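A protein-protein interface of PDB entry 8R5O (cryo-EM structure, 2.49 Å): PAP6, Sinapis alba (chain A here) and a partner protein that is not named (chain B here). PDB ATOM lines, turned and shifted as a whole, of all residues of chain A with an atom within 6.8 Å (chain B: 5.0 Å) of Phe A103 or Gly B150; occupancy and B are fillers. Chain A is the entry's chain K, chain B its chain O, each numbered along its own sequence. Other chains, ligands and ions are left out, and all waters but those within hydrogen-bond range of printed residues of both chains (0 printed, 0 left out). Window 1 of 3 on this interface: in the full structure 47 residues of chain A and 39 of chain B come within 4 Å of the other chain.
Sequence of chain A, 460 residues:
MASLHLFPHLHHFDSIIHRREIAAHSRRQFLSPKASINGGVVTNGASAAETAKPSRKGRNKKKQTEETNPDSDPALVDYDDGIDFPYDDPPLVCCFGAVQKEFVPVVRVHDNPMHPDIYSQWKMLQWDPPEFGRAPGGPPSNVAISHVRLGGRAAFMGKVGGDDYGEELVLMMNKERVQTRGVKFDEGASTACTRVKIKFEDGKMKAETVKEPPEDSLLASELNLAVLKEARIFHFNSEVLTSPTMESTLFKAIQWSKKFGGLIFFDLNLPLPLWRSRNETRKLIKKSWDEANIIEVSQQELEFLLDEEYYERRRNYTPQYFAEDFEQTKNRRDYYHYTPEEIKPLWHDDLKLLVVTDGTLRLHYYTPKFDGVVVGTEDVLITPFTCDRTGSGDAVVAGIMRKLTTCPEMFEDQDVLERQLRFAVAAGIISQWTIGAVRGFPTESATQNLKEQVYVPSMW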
ATOM      1  N   GLN A 100      13.741 -12.110  -7.467  1.00  0.00           N
ATOM      2  CA  GLN A 100      13.542 -13.349  -6.735  1.00  0.00           C
ATOM      3  C   GLN A 100      12.062 -13.692  -6.724  1.00  0.00           C
ATOM      4  O   GLN A 100      11.204 -12.819  -6.865  1.00  0.00           O
ATOM      5  CB  GLN A 100      14.065 -13.242  -5.298  1.00  0.00           C
ATOM      6  CG  GLN A 100      15.553 -12.960  -5.197  1.00  0.00           C
ATOM      7  CD  GLN A 100      15.927 -12.286  -3.894  1.00  0.00           C
ATOM      8  OE1 GLN A 100      15.202 -11.423  -3.400  1.00  0.00           O
ATOM      9  NE2 GLN A 100      17.061 -12.677  -3.329  1.00  0.00           N
ATOM     10  N   LYS A 101      11.774 -14.977  -6.559  1.00  0.00           N
ATOM     11  CA  LYS A 101      10.406 -15.446  -6.406  1.00  0.00           C
ATOM     12  C   LYS A 101      10.089 -15.516  -4.916  1.00  0.00           C
ATOM     13  O   LYS A 101      10.697 -16.307  -4.187  1.00  0.00           O
ATOM     14  CB  LYS A 101      10.224 -16.805  -7.078  1.00  0.00           C
ATOM     15  CG  LYS A 101       8.806 -17.089  -7.538  1.00  0.00           C
ATOM     16  CD  LYS A 101       8.691 -18.471  -8.158  1.00  0.00           C
ATOM     17  CE  LYS A 101       9.502 -18.575  -9.439  1.00  0.00           C
ATOM     18  NZ  LYS A 101       8.942 -17.722 -10.523  1.00  0.00           N
ATOM     19  N   GLU A 102       9.159 -14.669  -4.468  1.00  0.00           N
ATOM     20  CA  GLU A 102       8.764 -14.555  -3.060  1.00  0.00           C
ATOM     21  C   GLU A 102       9.961 -14.036  -2.270  1.00  0.00           C
ATOM     22  O   GLU A 102      10.382 -12.892  -2.517  1.00  0.00           O
ATOM     23  CB  GLU A 102       8.175 -15.886  -2.588  1.00  0.00           C
ATOM     24  CG  GLU A 102       6.676 -16.000  -2.800  1.00  0.00           C
ATOM     25  CD  GLU A 102       6.280 -15.905  -4.257  1.00  0.00           C
ATOM     26  OE1 GLU A 102       6.880 -16.624  -5.083  1.00  0.00           O
ATOM     27  OE2 GLU A 102       5.374 -15.108  -4.579  1.00  0.00           O
ATOM     28  N   PHE A 103      10.527 -14.801  -1.337  1.00  0.00           N
ATOM     29  CA  PHE A 103      11.667 -14.375  -0.527  1.00  0.00           C
ATOM     30  C   PHE A 103      11.398 -13.113   0.287  1.00  0.00           C
ATOM     31  O   PHE A 103      11.911 -12.038  -0.035  1.00  0.00           O
ATOM     32  CB  PHE A 103      12.921 -14.168  -1.377  1.00  0.00           C
ATOM     33  CG  PHE A 103      14.158 -13.966  -0.553  1.00  0.00           C
ATOM     34  CD1 PHE A 103      14.673 -15.009   0.200  1.00  0.00           C
ATOM     35  CD2 PHE A 103      14.789 -12.737  -0.502  1.00  0.00           C
ATOM     36  CE1 PHE A 103      15.801 -14.833   0.973  1.00  0.00           C
ATOM     37  CE2 PHE A 103      15.917 -12.553   0.271  1.00  0.00           C
ATOM     38  CZ  PHE A 103      16.426 -13.604   1.008  1.00  0.00           C
ATOM     39  N   VAL A 104      10.559 -13.221   1.311  1.00  0.00           N
ATOM     40  CA  VAL A 104      10.344 -12.123   2.252  1.00  0.00           C
ATOM     41  C   VAL A 104      11.654 -11.800   2.962  1.00  0.00           C
ATOM     42  O   VAL A 104      12.213 -12.664   3.652  1.00  0.00           O
ATOM     43  CB  VAL A 104       9.248 -12.479   3.267  1.00  0.00           C
ATOM     44  CG1 VAL A 104       8.886 -11.264   4.105  1.00  0.00           C
ATOM     45  CG2 VAL A 104       8.032 -13.037   2.550  1.00  0.00           C
ATOM     46  N   PRO A 105      12.176 -10.578   2.837  1.00  0.00           N
ATOM     47  CA  PRO A 105      13.462 -10.255   3.472  1.00  0.00           C
ATOM     48  C   PRO A 105      13.361  -9.924   4.954  1.00  0.00           C
ATOM     49  O   PRO A 105      14.269 -10.248   5.724  1.00  0.00           O
ATOM     50  CB  PRO A 105      13.945  -9.044   2.665  1.00  0.00           C
ATOM     51  CG  PRO A 105      12.691  -8.383   2.220  1.00  0.00           C
ATOM     52  CD  PRO A 105      11.690  -9.482   1.980  1.00  0.00           C
ATOM     53  N   VAL A 106      12.270  -9.285   5.368  1.00  0.00           N
ATOM     54  CA  VAL A 106      12.133  -8.794   6.738  1.00  0.00           C
ATOM     55  C   VAL A 106      11.758  -9.966   7.640  1.00  0.00           C
ATOM     56  O   VAL A 106      10.627 -10.457   7.598  1.00  0.00           O
ATOM     57  CB  VAL A 106      11.095  -7.670   6.830  1.00  0.00           C
ATOM     58  CG1 VAL A 106      10.941  -7.208   8.268  1.00  0.00           C
ATOM     59  CG2 VAL A 106      11.487  -6.511   5.928  1.00  0.00           C
ATOM     60  N   VAL A 107      12.704 -10.412   8.464  1.00  0.00           N
ATOM     61  CA  VAL A 107      12.510 -11.556   9.346  1.00  0.00           C
ATOM     62  C   VAL A 107      12.866 -11.140  10.766  1.00  0.00           C
ATOM     63  O   VAL A 107      13.993 -10.707  11.026  1.00  0.00           O
ATOM     64  CB  VAL A 107      13.355 -12.767   8.918  1.00  0.00           C
ATOM     65  CG1 VAL A 107      13.145 -13.923   9.887  1.00  0.00           C
ATOM     66  CG2 VAL A 107      13.013 -13.185   7.499  1.00  0.00           C
ATOM     67  N   GLY A 137       7.221  -6.344   2.519  1.00  0.00           N
ATOM     68  CA  GLY A 137       7.822  -6.059   1.236  1.00  0.00           C
ATOM     69  C   GLY A 137       8.530  -7.277   0.670  1.00  0.00           C
ATOM     70  O   GLY A 137       8.528  -8.363   1.246  1.00  0.00           O
ATOM     71  N   GLY A 138       9.148  -7.082  -0.490  1.00  0.00           N
ATOM     72  CA  GLY A 138       9.850  -8.154  -1.153  1.00  0.00           C
ATOM     73  C   GLY A 138      10.970  -7.671  -2.050  1.00  0.00           C
ATOM     74  O   GLY A 138      11.533  -6.589  -1.856  1.00  0.00           O
ATOM     75  N   PRO A 139      11.317  -8.473  -3.051  1.00  0.00           N
ATOM     76  CA  PRO A 139      12.391  -8.100  -3.973  1.00  0.00           C
ATOM     77  C   PRO A 139      11.963  -6.952  -4.870  1.00  0.00           C
ATOM     78  O   PRO A 139      10.761  -6.717  -5.059  1.00  0.00           O
ATOM     79  CB  PRO A 139      12.623  -9.387  -4.779  1.00  0.00           C
ATOM     80  CG  PRO A 139      11.311 -10.086  -4.734  1.00  0.00           C
ATOM     81  CD  PRO A 139      10.728  -9.782  -3.384  1.00  0.00           C
ATOM     82  N   GLU A 239      18.582  -4.572   0.627  1.00  0.00           N
ATOM     83  CA  GLU A 239      19.213  -5.870   0.424  1.00  0.00           C
ATOM     84  C   GLU A 239      20.510  -5.745  -0.364  1.00  0.00           C
ATOM     85  O   GLU A 239      21.424  -6.557  -0.184  1.00  0.00           O
ATOM     86  CB  GLU A 239      18.249  -6.823  -0.288  1.00  0.00           C
ATOM     87  CG  GLU A 239      17.062  -7.287   0.551  1.00  0.00           C
ATOM     88  CD  GLU A 239      15.939  -6.265   0.621  1.00  0.00           C
ATOM     89  OE1 GLU A 239      16.162  -5.162   1.161  1.00  0.00           O
ATOM     90  OE2 GLU A 239      14.832  -6.565   0.129  1.00  0.00           O
ATOM     91  N   PRO A 271      16.633  -6.549   5.609  1.00  0.00           N
ATOM     92  CA  PRO A 271      16.764  -8.006   5.715  1.00  0.00           C
ATOM     93  C   PRO A 271      17.139  -8.418   7.131  1.00  0.00           C
ATOM     94  O   PRO A 271      17.406  -7.593   8.004  1.00  0.00           O
ATOM     95  CB  PRO A 271      17.874  -8.337   4.716  1.00  0.00           C
ATOM     96  CG  PRO A 271      18.673  -7.092   4.629  1.00  0.00           C
ATOM     97  CD  PRO A 271      17.708  -5.954   4.799  1.00  0.00           C
ATOM     98  N   LEU A 272      17.155  -9.733   7.344  1.00  0.00           N
ATOM     99  CA  LEU A 272      17.410 -10.300   8.669  1.00  0.00           C
ATOM    100  C   LEU A 272      18.693  -9.794   9.325  1.00  0.00           C
ATOM    101  O   LEU A 272      18.640  -9.420  10.507  1.00  0.00           O
ATOM    102  CB  LEU A 272      17.404 -11.833   8.557  1.00  0.00           C
ATOM    103  CG  LEU A 272      17.170 -12.710   9.795  1.00  0.00           C
ATOM    104  CD1 LEU A 272      16.779 -14.112   9.364  1.00  0.00           C
ATOM    105  CD2 LEU A 272      18.386 -12.770  10.706  1.00  0.00           C
ATOM    106  N   PRO A 273      19.855  -9.760   8.655  1.00  0.00           N
ATOM    107  CA  PRO A 273      21.070  -9.298   9.352  1.00  0.00           C
ATOM    108  C   PRO A 273      20.983  -7.873   9.875  1.00  0.00           C
ATOM    109  O   PRO A 273      21.564  -7.572  10.925  1.00  0.00           O
ATOM    110  CB  PRO A 273      22.160  -9.437   8.280  1.00  0.00           C
ATOM    111  CG  PRO A 273      21.639 -10.444   7.339  1.00  0.00           C
ATOM    112  CD  PRO A 273      20.165 -10.221   7.290  1.00  0.00           C
ATOM    113  N   THR A 390       1.826 -11.380   1.845  1.00  0.00           N
ATOM    114  CA  THR A 390       3.094 -11.246   1.141  1.00  0.00           C
ATOM    115  C   THR A 390       2.920 -10.453  -0.148  1.00  0.00           C
ATOM    116  O   THR A 390       2.023 -10.731  -0.949  1.00  0.00           O
ATOM    117  CB  THR A 390       3.674 -12.629   0.837  1.00  0.00           C
ATOM    118  OG1 THR A 390       3.956 -13.308   2.066  1.00  0.00           O
ATOM    119  CG2 THR A 390       4.953 -12.512   0.023  1.00  0.00           C
ATOM    120  N   PRO B 110       5.029 -17.612   2.125  1.00  0.00           N
ATOM    121  CA  PRO B 110       5.718 -18.508   1.178  1.00  0.00           C
ATOM    122  C   PRO B 110       6.210 -19.807   1.792  1.00  0.00           C
ATOM    123  O   PRO B 110       6.427 -20.774   1.053  1.00  0.00           O
ATOM    124  CB  PRO B 110       6.888 -17.649   0.680  1.00  0.00           C
ATOM    125  CG  PRO B 110       6.393 -16.264   0.799  1.00  0.00           C
ATOM    126  CD  PRO B 110       5.547 -16.235   2.036  1.00  0.00           C
ATOM    127  N   VAL B 148      21.521 -16.399   6.785  1.00  0.00           N
ATOM    128  CA  VAL B 148      20.152 -16.352   6.286  1.00  0.00           C
ATOM    129  C   VAL B 148      19.718 -14.894   6.194  1.00  0.00           C
ATOM    130  O   VAL B 148      19.677 -14.178   7.201  1.00  0.00           O
ATOM    131  CB  VAL B 148      19.208 -17.161   7.184  1.00  0.00           C
ATOM    132  CG1 VAL B 148      17.769 -16.994   6.726  1.00  0.00           C
ATOM    133  CG2 VAL B 148      19.600 -18.630   7.181  1.00  0.00           C
ATOM    134  N   ARG B 149      19.405 -14.446   4.979  1.00  0.00           N
ATOM    135  CA  ARG B 149      18.973 -13.076   4.739  1.00  0.00           C
ATOM    136  C   ARG B 149      17.462 -12.939   4.622  1.00  0.00           C
ATOM    137  O   ARG B 149      16.957 -11.813   4.600  1.00  0.00           O
ATOM    138  CB  ARG B 149      19.630 -12.527   3.465  1.00  0.00           C
ATOM    139  CG  ARG B 149      21.143 -12.449   3.528  1.00  0.00           C
ATOM    140  CD  ARG B 149      21.715 -11.796   2.278  1.00  0.00           C
ATOM    141  NE  ARG B 149      21.416 -12.560   1.073  1.00  0.00           N
ATOM    142  CZ  ARG B 149      21.762 -12.194  -0.154  1.00  0.00           C
ATOM    143  NH1 ARG B 149      22.419 -11.069  -0.381  1.00  0.00           N
ATOM    144  NH2 ARG B 149      21.440 -12.977  -1.180  1.00  0.00           N
ATOM    145  N   GLY B 150      16.739 -14.048   4.553  1.00  0.00           N
ATOM    146  CA  GLY B 150      15.298 -14.013   4.434  1.00  0.00           C
ATOM    147  C   GLY B 150      14.761 -15.421   4.319  1.00  0.00           C
ATOM    148  O   GLY B 150      15.505 -16.404   4.372  1.00  0.00           O
ATOM    149  N   LEU B 151      13.448 -15.501   4.149  1.00  0.00           N
ATOM    150  CA  LEU B 151      12.765 -16.780   4.072  1.00  0.00           C
ATOM    151  C   LEU B 151      11.942 -16.856   2.797  1.00  0.00           C
ATOM    152  O   LEU B 151      11.387 -15.848   2.354  1.00  0.00           O
ATOM    153  CB  LEU B 151      11.851 -16.984   5.288  1.00  0.00           C
ATOM    154  CG  LEU B 151      12.538 -16.938   6.654  1.00  0.00           C
ATOM    155  CD1 LEU B 151      11.523 -17.063   7.779  1.00  0.00           C
ATOM    156  CD2 LEU B 151      13.585 -18.029   6.753  1.00  0.00           C
ATOM    157  N   PRO B 152      11.835 -18.047   2.186  1.00  0.00           N
ATOM    158  CA  PRO B 152      12.468 -19.325   2.555  1.00  0.00           C
ATOM    159  C   PRO B 152      13.920 -19.441   2.095  1.00  0.00           C
ATOM    160  O   PRO B 152      14.291 -18.927   1.044  1.00  0.00           O
ATOM    161  CB  PRO B 152      11.573 -20.352   1.853  1.00  0.00           C
ATOM    162  CG  PRO B 152      11.129 -19.641   0.614  1.00  0.00           C
ATOM    163  CD  PRO B 152      10.921 -18.208   1.040  1.00  0.00           C
ATOM    164  N   THR B 153      14.759 -20.125   2.866  1.00  0.00           N
ATOM    165  CA  THR B 153      16.165 -20.323   2.536  1.00  0.00           C
ATOM    166  C   THR B 153      16.505 -21.796   2.695  1.00  0.00           C
ATOM    167  O   THR B 153      16.125 -22.419   3.690  1.00  0.00           O
ATOM    168  CB  THR B 153      17.071 -19.466   3.429  1.00  0.00           C
ATOM    169  OG1 THR B 153      16.833 -18.078   3.164  1.00  0.00           O
ATOM    170  CG2 THR B 153      18.535 -19.779   3.175  1.00  0.00           C
ATOM    171  N   GLU B 169      17.808 -19.028  -2.255  1.00  0.00           N
ATOM    172  CA  GLU B 169      16.816 -18.098  -1.740  1.00  0.00           C
ATOM    173  C   GLU B 169      15.589 -18.098  -2.641  1.00  0.00           C
ATOM    174  O   GLU B 169      15.710 -18.110  -3.870  1.00  0.00           O
ATOM    175  CB  GLU B 169      17.385 -16.680  -1.635  1.00  0.00           C
ATOM    176  CG  GLU B 169      18.582 -16.559  -0.713  1.00  0.00           C
ATOM    177  CD  GLU B 169      19.162 -15.160  -0.696  1.00  0.00           C
ATOM    178  OE1 GLU B 169      18.818 -14.361  -1.593  1.00  0.00           O
ATOM    179  OE2 GLU B 169      19.963 -14.858   0.213  1.00  0.00           O
ATOM    180  N   GLY B 170      14.413 -18.084  -2.023  1.00  0.00           N
ATOM    181  CA  GLY B 170      13.164 -18.008  -2.748  1.00  0.00           C
ATOM    182  C   GLY B 170      12.554 -19.368  -3.035  1.00  0.00           C
ATOM    183  O   GLY B 170      13.142 -20.425  -2.795  1.00  0.00           O
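Printed residues of chain A that touch a printed residue of chain B: Gln A100, Lys A101, Glu A102, Phe A103, Val A104, Pro A105, Val A107, Pro A271, Leu A272, Pro A273 and Thr A390.
Hydrophobic or aromatic side chains of chain A within 4 Å of the printed part of chain B: Phe A103, Val A107, Pro A271, Leu A272 and Pro A273.
Of the 9 printed residues of chain B, 7 touch a printed residue of chain A.
Printed residues of chain B that touch a printed residue of chain A: Pro B110, Val B148, Arg B149, Gly B150, Leu B151, Glu B169 and Gly B170.
Among the printed residues, 18 pairs touch across the chains.
Among the printed residues, no Asp or Glu carboxylate lies within 4 Å of a Lys or Arg side-chain nitrogen of the other chain.
Lys A101 touches Gly B170 (O to CA, 3.3 Å).
Phe A103 touches Arg B149.
Leu B151 touches Phe A103 (O to CA, 3.2 Å).
Phe A103 touches Glu B169.
N of Gly B170 touches CD1 of Phe A103, 3.8 Å away.
O of Val A104 touches CA of Gly B150, 3.5 Å away.
Val A107 touches Gly B150 (CG2 to CA, 3.9 Å).
CG of Leu B151 touches CG2 of Val A107 (3.9 Å).
Pro A271 touches Arg B149.
OG1 of Thr A390 touches CD of Pro B110, at 3.3 Å.
Phe A103 touches five residues of chain B.
Of chain A, only Phe A103, Val A104 and Val A107 come within 4 Å of Gly B150.
Printed residues of chain B within 4 Å of Leu A272: Val B148 and Arg B149.
Of the printed residues of chain B, Gln A100 touches Glu B169 (3.0 Å).
Printed residues of chain B within 4 Å of Pro A105: Arg B149.
Of the printed residues of chain A, Leu B151 touches Phe A103 (3.2 Å), Val A104 (2.9 Å) and Val A107 (3.9 Å).
Gly A138 touches none of the printed residues of chain B.
Thr B153 touches none of the printed residues of chain A.
The nearest printed residue of chain B that does not touch Phe A103 is Pro B152 (4.03 Å).
The nearest residue of chain A that does not touch Gly B150 is Pro A105 (4.1 Å).
The nearest printed residue of chain B that does not touch Pro A105 is Gly B150 (4.1 Å).
O of Pro A105 sits at hydrogen-bond distance from N of Leu A272, 3.3 Å away.
The guanidinium group (NH2) of Arg B149 lies within salt-bridge range of the side-chain carboxylate (OE2) of Glu B169 (2.8 Å).
The backbone carbonyl oxygen (O) of Gly B150 is in hydrogen-bond range of the side-chain hydroxyl (OG1) of Thr B153, 2.5 Å away.
O of Pro B152 lies within hydrogen-bond range of N of Gly B170, at 3.2 Å.
O of Pro A105 lies close to O of Arg B149 (3.3 Å).
The backbone carbonyl oxygen (O) of Leu B151 lies within hydrogen-bond range of the backbone NH (N) of Val A104 (2.9 Å).
The backbone NH (N) of Leu A272 sits at hydrogen-bond distance from the backbone carbonyl oxygen (O) of Arg B149 (3.4 Å).
NE2 of Gln A100 lies within hydrogen-bond range of OE1 of Glu B169 (3.0 Å).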
